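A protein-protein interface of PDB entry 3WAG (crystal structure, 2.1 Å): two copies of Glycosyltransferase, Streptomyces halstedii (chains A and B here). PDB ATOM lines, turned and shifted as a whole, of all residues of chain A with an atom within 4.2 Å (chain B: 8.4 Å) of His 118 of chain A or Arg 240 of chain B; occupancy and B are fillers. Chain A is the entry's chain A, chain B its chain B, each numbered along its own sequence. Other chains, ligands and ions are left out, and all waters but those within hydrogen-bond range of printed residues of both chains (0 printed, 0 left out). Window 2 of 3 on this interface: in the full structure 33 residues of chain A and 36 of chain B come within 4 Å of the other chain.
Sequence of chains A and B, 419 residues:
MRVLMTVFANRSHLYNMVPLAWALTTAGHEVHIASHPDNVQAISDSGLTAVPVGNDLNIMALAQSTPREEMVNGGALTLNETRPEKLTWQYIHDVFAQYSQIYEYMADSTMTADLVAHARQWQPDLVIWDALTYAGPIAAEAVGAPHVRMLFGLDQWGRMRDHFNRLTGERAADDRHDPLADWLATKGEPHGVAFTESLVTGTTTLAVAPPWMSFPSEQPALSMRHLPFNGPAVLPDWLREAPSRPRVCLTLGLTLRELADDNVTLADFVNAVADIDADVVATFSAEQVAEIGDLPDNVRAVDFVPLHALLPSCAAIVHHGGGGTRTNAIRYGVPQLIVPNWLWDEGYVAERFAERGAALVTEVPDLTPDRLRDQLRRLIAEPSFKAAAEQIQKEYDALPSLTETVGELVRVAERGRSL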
ATOM      1  N   LEU A   4      10.790 -16.108  29.866  1.00  0.00           N
ATOM      2  CA  LEU A   4      11.767 -16.461  28.857  1.00  0.00           C
ATOM      3  C   LEU A   4      11.186 -17.600  27.980  1.00  0.00           C
ATOM      4  O   LEU A   4      11.152 -18.769  28.366  1.00  0.00           O
ATOM      5  CB  LEU A   4      13.092 -16.892  29.541  1.00  0.00           C
ATOM      6  CG  LEU A   4      14.237 -17.288  28.616  1.00  0.00           C
ATOM      7  CD1 LEU A   4      14.523 -16.211  27.565  1.00  0.00           C
ATOM      8  CD2 LEU A   4      15.504 -17.663  29.384  1.00  0.00           C
ATOM      9  N   HIS A  32      10.651 -12.319  26.654  1.00  0.00           N
ATOM     10  CA  HIS A  32      11.748 -12.537  25.701  1.00  0.00           C
ATOM     11  C   HIS A  32      11.569 -13.854  24.960  1.00  0.00           C
ATOM     12  O   HIS A  32      11.221 -14.921  25.602  1.00  0.00           O
ATOM     13  CB  HIS A  32      13.116 -12.606  26.379  1.00  0.00           C
ATOM     14  CG  HIS A  32      13.539 -11.341  27.055  1.00  0.00           C
ATOM     15  ND1 HIS A  32      14.687 -11.255  27.788  1.00  0.00           N
ATOM     16  CD2 HIS A  32      12.935 -10.091  27.116  1.00  0.00           C
ATOM     17  CE1 HIS A  32      14.820 -10.004  28.282  1.00  0.00           C
ATOM     18  NE2 HIS A  32      13.730  -9.287  27.879  1.00  0.00           N
ATOM     19  N   VAL A  51      15.904 -12.355  21.530  1.00  0.00           N
ATOM     20  CA  VAL A  51      17.146 -12.553  22.207  1.00  0.00           C
ATOM     21  C   VAL A  51      17.867 -13.608  21.405  1.00  0.00           C
ATOM     22  O   VAL A  51      17.522 -14.778  21.455  1.00  0.00           O
ATOM     23  CB  VAL A  51      16.967 -12.969  23.700  1.00  0.00           C
ATOM     24  CG1 VAL A  51      18.309 -13.308  24.306  1.00  0.00           C
ATOM     25  CG2 VAL A  51      16.302 -11.838  24.510  1.00  0.00           C
ATOM     26  N   PRO A  52      18.871 -13.185  20.608  1.00  0.00           N
ATOM     27  CA  PRO A  52      19.660 -14.178  19.844  1.00  0.00           C
ATOM     28  C   PRO A  52      20.471 -15.023  20.791  1.00  0.00           C
ATOM     29  O   PRO A  52      21.068 -14.494  21.750  1.00  0.00           O
ATOM     30  CB  PRO A  52      20.640 -13.310  19.014  1.00  0.00           C
ATOM     31  CG  PRO A  52      20.718 -12.008  19.773  1.00  0.00           C
ATOM     32  CD  PRO A  52      19.385 -11.805  20.467  1.00  0.00           C
ATOM     33  N   ASP A 114      24.416 -20.039  25.786  1.00  0.00           N
ATOM     34  CA  ASP A 114      23.920 -18.641  25.715  1.00  0.00           C
ATOM     35  C   ASP A 114      22.583 -18.417  26.466  1.00  0.00           C
ATOM     36  O   ASP A 114      22.402 -17.414  27.158  1.00  0.00           O
ATOM     37  CB  ASP A 114      23.760 -18.149  24.275  1.00  0.00           C
ATOM     38  CG  ASP A 114      25.093 -18.039  23.510  1.00  0.00           C
ATOM     39  OD1 ASP A 114      26.164 -18.123  24.136  1.00  0.00           O
ATOM     40  OD2 ASP A 114      25.059 -17.895  22.256  1.00  0.00           O
ATOM     41  N   LEU A 115      21.656 -19.359  26.315  1.00  0.00           N
ATOM     42  CA  LEU A 115      20.351 -19.229  26.933  1.00  0.00           C
ATOM     43  C   LEU A 115      20.482 -19.365  28.431  1.00  0.00           C
ATOM     44  O   LEU A 115      19.780 -18.678  29.164  1.00  0.00           O
ATOM     45  CB  LEU A 115      19.371 -20.279  26.409  1.00  0.00           C
ATOM     46  CG  LEU A 115      17.898 -20.096  26.906  1.00  0.00           C
ATOM     47  CD1 LEU A 115      17.210 -18.931  26.315  1.00  0.00           C
ATOM     48  CD2 LEU A 115      17.071 -21.342  26.575  1.00  0.00           C
ATOM     49  N   VAL A 116      21.349 -20.263  28.892  1.00  0.00           N
ATOM     50  CA  VAL A 116      21.606 -20.388  30.346  1.00  0.00           C
ATOM     51  C   VAL A 116      22.210 -19.079  30.895  1.00  0.00           C
ATOM     52  O   VAL A 116      21.833 -18.615  31.967  1.00  0.00           O
ATOM     53  CB  VAL A 116      22.551 -21.560  30.697  1.00  0.00           C
ATOM     54  CG1 VAL A 116      23.150 -21.360  32.074  1.00  0.00           C
ATOM     55  CG2 VAL A 116      21.835 -22.893  30.649  1.00  0.00           C
ATOM     56  N   ALA A 117      23.146 -18.482  30.150  1.00  0.00           N
ATOM     57  CA  ALA A 117      23.810 -17.263  30.652  1.00  0.00           C
ATOM     58  C   ALA A 117      22.814 -16.108  30.736  1.00  0.00           C
ATOM     59  O   ALA A 117      22.832 -15.347  31.693  1.00  0.00           O
ATOM     60  CB  ALA A 117      25.029 -16.906  29.771  1.00  0.00           C
ATOM     61  N   HIS A 118      21.899 -16.022  29.758  1.00  0.00           N
ATOM     62  CA  HIS A 118      20.829 -15.026  29.763  1.00  0.00           C
ATOM     63  C   HIS A 118      19.832 -15.271  30.878  1.00  0.00           C
ATOM     64  O   HIS A 118      19.436 -14.348  31.590  1.00  0.00           O
ATOM     65  CB  HIS A 118      20.111 -14.983  28.419  1.00  0.00           C
ATOM     66  CG  HIS A 118      19.017 -13.933  28.361  1.00  0.00           C
ATOM     67  ND1 HIS A 118      19.291 -12.620  28.282  1.00  0.00           N
ATOM     68  CD2 HIS A 118      17.616 -14.049  28.333  1.00  0.00           C
ATOM     69  CE1 HIS A 118      18.139 -11.908  28.238  1.00  0.00           C
ATOM     70  NE2 HIS A 118      17.107 -12.782  28.263  1.00  0.00           N
ATOM     71  N   ALA A 119      19.412 -16.515  31.070  1.00  0.00           N
ATOM     72  CA  ALA A 119      18.593 -16.825  32.260  1.00  0.00           C
ATOM     73  C   ALA A 119      19.296 -16.356  33.553  1.00  0.00           C
ATOM     74  O   ALA A 119      18.683 -15.711  34.409  1.00  0.00           O
ATOM     75  CB  ALA A 119      18.283 -18.304  32.321  1.00  0.00           C
ATOM     76  N   ARG A 120      20.591 -16.615  33.671  1.00  0.00           N
ATOM     77  CA  ARG A 120      21.295 -16.254  34.940  1.00  0.00           C
ATOM     78  C   ARG A 120      21.292 -14.787  35.198  1.00  0.00           C
ATOM     79  O   ARG A 120      21.011 -14.380  36.316  1.00  0.00           O
ATOM     80  CB  ARG A 120      22.708 -16.725  34.975  1.00  0.00           C
ATOM     81  CG  ARG A 120      22.862 -18.180  35.287  1.00  0.00           C
ATOM     82  CD  ARG A 120      24.334 -18.465  35.541  1.00  0.00           C
ATOM     83  NE  ARG A 120      24.638 -19.868  35.285  1.00  0.00           N
ATOM     84  CZ  ARG A 120      24.094 -20.875  35.955  1.00  0.00           C
ATOM     85  NH1 ARG A 120      23.201 -20.638  36.920  1.00  0.00           N
ATOM     86  NH2 ARG A 120      24.419 -22.114  35.652  1.00  0.00           N
ATOM     87  N   GLN A 121      21.557 -13.991  34.156  1.00  0.00           N
ATOM     88  CA  GLN A 121      21.497 -12.540  34.244  1.00  0.00           C
ATOM     89  C   GLN A 121      20.063 -11.966  34.344  1.00  0.00           C
ATOM     90  O   GLN A 121      19.819 -11.043  35.132  1.00  0.00           O
ATOM     91  CB  GLN A 121      22.240 -11.909  33.057  1.00  0.00           C
ATOM     92  CG  GLN A 121      22.191 -10.393  33.035  1.00  0.00           C
ATOM     93  CD  GLN A 121      22.733  -9.769  34.331  1.00  0.00           C
ATOM     94  OE1 GLN A 121      23.841 -10.091  34.781  1.00  0.00           O
ATOM     95  NE2 GLN A 121      21.949  -8.880  34.940  1.00  0.00           N
ATOM     96  N   TRP A 122      19.126 -12.473  33.539  1.00  0.00           N
ATOM     97  CA  TRP A 122      17.738 -11.938  33.513  1.00  0.00           C
ATOM     98  C   TRP A 122      16.807 -12.474  34.594  1.00  0.00           C
ATOM     99  O   TRP A 122      15.782 -11.848  34.925  1.00  0.00           O
ATOM    100  CB  TRP A 122      17.092 -12.170  32.140  1.00  0.00           C
ATOM    101  CG  TRP A 122      15.854 -11.351  31.879  1.00  0.00           C
ATOM    102  CD1 TRP A 122      15.696 -10.002  32.087  1.00  0.00           C
ATOM    103  CD2 TRP A 122      14.557 -11.784  31.309  1.00  0.00           C
ATOM    104  NE1 TRP A 122      14.440  -9.598  31.750  1.00  0.00           N
ATOM    105  CE2 TRP A 122      13.728 -10.599  31.246  1.00  0.00           C
ATOM    106  CE3 TRP A 122      14.051 -12.979  30.837  1.00  0.00           C
ATOM    107  CZ2 TRP A 122      12.437 -10.617  30.745  1.00  0.00           C
ATOM    108  CZ3 TRP A 122      12.722 -13.012  30.390  1.00  0.00           C
ATOM    109  CH2 TRP A 122      11.943 -11.856  30.322  1.00  0.00           C
ATOM    110  N   VAL B 234      15.075  -6.335  19.078  1.00  0.00           N
ATOM    111  CA  VAL B 234      16.133  -7.331  19.175  1.00  0.00           C
ATOM    112  C   VAL B 234      17.063  -6.832  20.265  1.00  0.00           C
ATOM    113  O   VAL B 234      17.570  -5.734  20.159  1.00  0.00           O
ATOM    114  CB  VAL B 234      16.924  -7.435  17.872  1.00  0.00           C
ATOM    115  CG1 VAL B 234      18.034  -8.467  18.011  1.00  0.00           C
ATOM    116  CG2 VAL B 234      16.016  -7.790  16.691  1.00  0.00           C
ATOM    117  N   LEU B 235      17.266  -7.601  21.329  1.00  0.00           N
ATOM    118  CA  LEU B 235      18.111  -7.143  22.415  1.00  0.00           C
ATOM    119  C   LEU B 235      19.548  -7.270  22.013  1.00  0.00           C
ATOM    120  O   LEU B 235      19.929  -8.331  21.546  1.00  0.00           O
ATOM    121  CB  LEU B 235      17.864  -7.935  23.683  1.00  0.00           C
ATOM    122  CG  LEU B 235      16.881  -7.340  24.701  1.00  0.00           C
ATOM    123  CD1 LEU B 235      15.496  -7.139  24.134  1.00  0.00           C
ATOM    124  CD2 LEU B 235      16.795  -8.222  25.928  1.00  0.00           C
ATOM    125  N   PRO B 236      20.342  -6.180  22.152  1.00  0.00           N
ATOM    126  CA  PRO B 236      21.744  -6.316  21.746  1.00  0.00           C
ATOM    127  C   PRO B 236      22.584  -6.836  22.911  1.00  0.00           C
ATOM    128  O   PRO B 236      22.162  -6.753  24.067  1.00  0.00           O
ATOM    129  CB  PRO B 236      22.162  -4.875  21.323  1.00  0.00           C
ATOM    130  CG  PRO B 236      21.157  -3.960  21.957  1.00  0.00           C
ATOM    131  CD  PRO B 236      20.026  -4.796  22.559  1.00  0.00           C
ATOM    132  N   ASP B 237      23.761  -7.360  22.599  1.00  0.00           N
ATOM    133  CA  ASP B 237      24.622  -7.938  23.591  1.00  0.00           C
ATOM    134  C   ASP B 237      24.863  -6.959  24.716  1.00  0.00           C
ATOM    135  O   ASP B 237      24.877  -7.331  25.883  1.00  0.00           O
ATOM    136  CB  ASP B 237      25.964  -8.302  22.945  1.00  0.00           C
ATOM    137  CG  ASP B 237      25.933  -9.650  22.277  1.00  0.00           C
ATOM    138  OD1 ASP B 237      24.835 -10.231  22.178  1.00  0.00           O
ATOM    139  OD2 ASP B 237      27.002 -10.140  21.842  1.00  0.00           O
ATOM    140  N   TRP B 238      25.055  -5.691  24.382  1.00  0.00           N
ATOM    141  CA  TRP B 238      25.535  -4.787  25.420  1.00  0.00           C
ATOM    142  C   TRP B 238      24.472  -4.555  26.487  1.00  0.00           C
ATOM    143  O   TRP B 238      24.831  -4.458  27.661  1.00  0.00           O
ATOM    144  CB  TRP B 238      26.112  -3.513  24.807  1.00  0.00           C
ATOM    145  CG  TRP B 238      25.089  -2.719  24.050  1.00  0.00           C
ATOM    146  CD1 TRP B 238      24.895  -2.650  22.679  1.00  0.00           C
ATOM    147  CD2 TRP B 238      24.093  -1.818  24.636  1.00  0.00           C
ATOM    148  NE1 TRP B 238      23.834  -1.822  22.387  1.00  0.00           N
ATOM    149  CE2 TRP B 238      23.312  -1.295  23.528  1.00  0.00           C
ATOM    150  CE3 TRP B 238      23.749  -1.463  25.946  1.00  0.00           C
ATOM    151  CZ2 TRP B 238      22.286  -0.401  23.721  1.00  0.00           C
ATOM    152  CZ3 TRP B 238      22.702  -0.569  26.134  1.00  0.00           C
ATOM    153  CH2 TRP B 238      21.989  -0.046  25.048  1.00  0.00           C
ATOM    154  N   LEU B 239      23.169  -4.538  26.110  1.00  0.00           N
ATOM    155  CA  LEU B 239      22.057  -4.410  27.085  1.00  0.00           C
ATOM    156  C   LEU B 239      21.885  -5.628  27.965  1.00  0.00           C
ATOM    157  O   LEU B 239      21.109  -5.607  28.918  1.00  0.00           O
ATOM    158  CB  LEU B 239      20.710  -4.235  26.417  1.00  0.00           C
ATOM    159  CG  LEU B 239      19.893  -2.942  26.543  1.00  0.00           C
ATOM    160  CD1 LEU B 239      18.563  -3.113  25.824  1.00  0.00           C
ATOM    161  CD2 LEU B 239      19.755  -2.409  27.952  1.00  0.00           C
ATOM    162  N   ARG B 240      22.542  -6.723  27.612  1.00  0.00           N
ATOM    163  CA  ARG B 240      22.184  -7.979  28.256  1.00  0.00           C
ATOM    164  C   ARG B 240      23.120  -8.378  29.423  1.00  0.00           C
ATOM    165  O   ARG B 240      22.793  -9.264  30.230  1.00  0.00           O
ATOM    166  CB  ARG B 240      21.941  -9.078  27.196  1.00  0.00           C
ATOM    167  CG  ARG B 240      20.560  -8.916  26.570  1.00  0.00           C
ATOM    168  CD  ARG B 240      20.121 -10.098  25.742  1.00  0.00           C
ATOM    169  NE  ARG B 240      20.740 -10.069  24.422  1.00  0.00           N
ATOM    170  CZ  ARG B 240      21.748 -10.843  24.019  1.00  0.00           C
ATOM    171  NH1 ARG B 240      22.289 -11.801  24.823  1.00  0.00           N
ATOM    172  NH2 ARG B 240      22.171 -10.667  22.767  1.00  0.00           N
ATOM    173  N   GLU B 241      24.237  -7.661  29.541  1.00  0.00           N
ATOM    174  CA  GLU B 241      25.190  -7.837  30.646  1.00  0.00           C
ATOM    175  C   GLU B 241      24.763  -7.017  31.834  1.00  0.00           C
ATOM    176  O   GLU B 241      23.903  -6.157  31.709  1.00  0.00           O
ATOM    177  CB  GLU B 241      26.568  -7.377  30.217  1.00  0.00           C
ATOM    178  CG  GLU B 241      26.783  -7.494  28.721  1.00  0.00           C
ATOM    179  CD  GLU B 241      27.901  -6.604  28.234  1.00  0.00           C
ATOM    180  OE1 GLU B 241      28.339  -5.729  29.016  1.00  0.00           O
ATOM    181  OE2 GLU B 241      28.343  -6.781  27.077  1.00  0.00           O
ATOM    182  N   ALA B 242      25.368  -7.282  32.991  1.00  0.00           N
ATOM    183  CA  ALA B 242      25.026  -6.578  34.232  1.00  0.00           C
ATOM    184  C   ALA B 242      25.431  -5.112  34.136  1.00  0.00           C
ATOM    185  O   ALA B 242      26.486  -4.789  33.607  1.00  0.00           O
ATOM    186  CB  ALA B 242      25.707  -7.236  35.426  1.00  0.00           C
ATOM    187  N   PRO B 243      24.583  -4.213  34.624  1.00  0.00           N
ATOM    188  CA  PRO B 243      25.017  -2.807  34.620  1.00  0.00           C
ATOM    189  C   PRO B 243      26.147  -2.488  35.645  1.00  0.00           C
ATOM    190  O   PRO B 243      26.052  -2.857  36.803  1.00  0.00           O
ATOM    191  CB  PRO B 243      23.725  -2.027  34.914  1.00  0.00           C
ATOM    192  CG  PRO B 243      22.742  -3.039  35.433  1.00  0.00           C
ATOM    193  CD  PRO B 243      23.158  -4.394  34.951  1.00  0.00           C
ATOM    194  N   ARG B 247      22.470   4.226  34.929  1.00  0.00           N
ATOM    195  CA  ARG B 247      22.314   4.595  33.496  1.00  0.00           C
ATOM    196  C   ARG B 247      21.287   5.676  33.284  1.00  0.00           C
ATOM    197  O   ARG B 247      20.359   5.815  34.081  1.00  0.00           O
ATOM    198  CB  ARG B 247      21.864   3.404  32.664  1.00  0.00           C
ATOM    199  CG  ARG B 247      22.980   2.535  32.198  1.00  0.00           C
ATOM    200  CD  ARG B 247      22.442   1.182  31.835  1.00  0.00           C
ATOM    201  NE  ARG B 247      23.499   0.364  31.258  1.00  0.00           N
ATOM    202  CZ  ARG B 247      23.352  -0.915  30.938  1.00  0.00           C
ATOM    203  NH1 ARG B 247      22.192  -1.524  31.146  1.00  0.00           N
ATOM    204  NH2 ARG B 247      24.357  -1.581  30.393  1.00  0.00           N
ATOM    205  N   ALA B 309      13.332  -2.719  27.396  1.00  0.00           N
ATOM    206  CA  ALA B 309      14.536  -3.476  27.802  1.00  0.00           C
ATOM    207  C   ALA B 309      15.571  -2.620  28.498  1.00  0.00           C
ATOM    208  O   ALA B 309      16.296  -3.151  29.299  1.00  0.00           O
ATOM    209  CB  ALA B 309      15.196  -4.273  26.669  1.00  0.00           C
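Printed residues of chain B within 4 Å of His 32 of chain A: Leu 235 (3.6 Å). Printed residues of chain B within 4 Å of Pro 52 of chain A: Leu 235 and Arg 240. No residue of chain B comes within 4 Å of Ala 117 of chain A. Of chain B, only Arg 240 (3.7 Å) comes within 4 Å of His 118 of chain A. Of the printed residues of chain B, Gln 121 of chain A touches Arg 240 (3.1 Å) and Ala 242 (3.5 Å). Arg 240 of chain B touches just these residues of chain A: Val 51 (3.96 Å), Pro 52 (3.6 Å), His 118 (3.7 Å) and Gln 121 (3.1 Å). Of the printed residues of chain A, Ala 242 of chain B touches Gln 121. The nearest printed residue of chain B that does not touch Val 51 of chain A is Val 234 of chain B (5.6 Å).
A ring nitrogen (NE2) of His 118 of chain A sits at hydrogen-bond distance from a ring nitrogen (ND1) of His 32 of chain A (2.9 Å). O of Leu 235 of chain B sits at hydrogen-bond distance from NE of Arg 240 of chain B (3.5 Å). The side-chain carboxylate (OD1) of Asp 237 of chain B lies within salt-bridge range of the guanidinium group (NH2) of Arg 240 of chain B (2.8 Å).
Among the printed residues, merely in contact across the chains: Gln 121 of chain A with Arg 240 of chain B (3.1 Å), Gln 121 of chain A with Ala 242 of chain B (3.5 Å), His 32 of chain A with Leu 235 of chain B (3.6 Å), Pro 52 of chain A with Arg 240 of chain B (3.6 Å), His 118 of chain A with Arg 240 of chain B (3.7 Å), Pro 52 of chain A with Leu 235 of chain B (3.7 Å), Val 51 of chain A with Leu 235 of chain B (3.9 Å) and Val 51 of chain A with Arg 240 of chain B (3.96 Å).
No position is printed for both chains.
Printed residues of chain A that touch a printed residue of chain B: His 32, Val 51, Pro 52, His 118 and Gln 121. Hydrophobic or aromatic side chains of chain A within 4 Å of the printed part of chain B: His 32, Val 51, Pro 52 and His 118. Among the printed residues, 8 pairs touch across the chains. Among the printed residues, no Asp or Glu carboxylate lies within 4 Å of a Lys or Arg side-chain nitrogen of the other chain.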
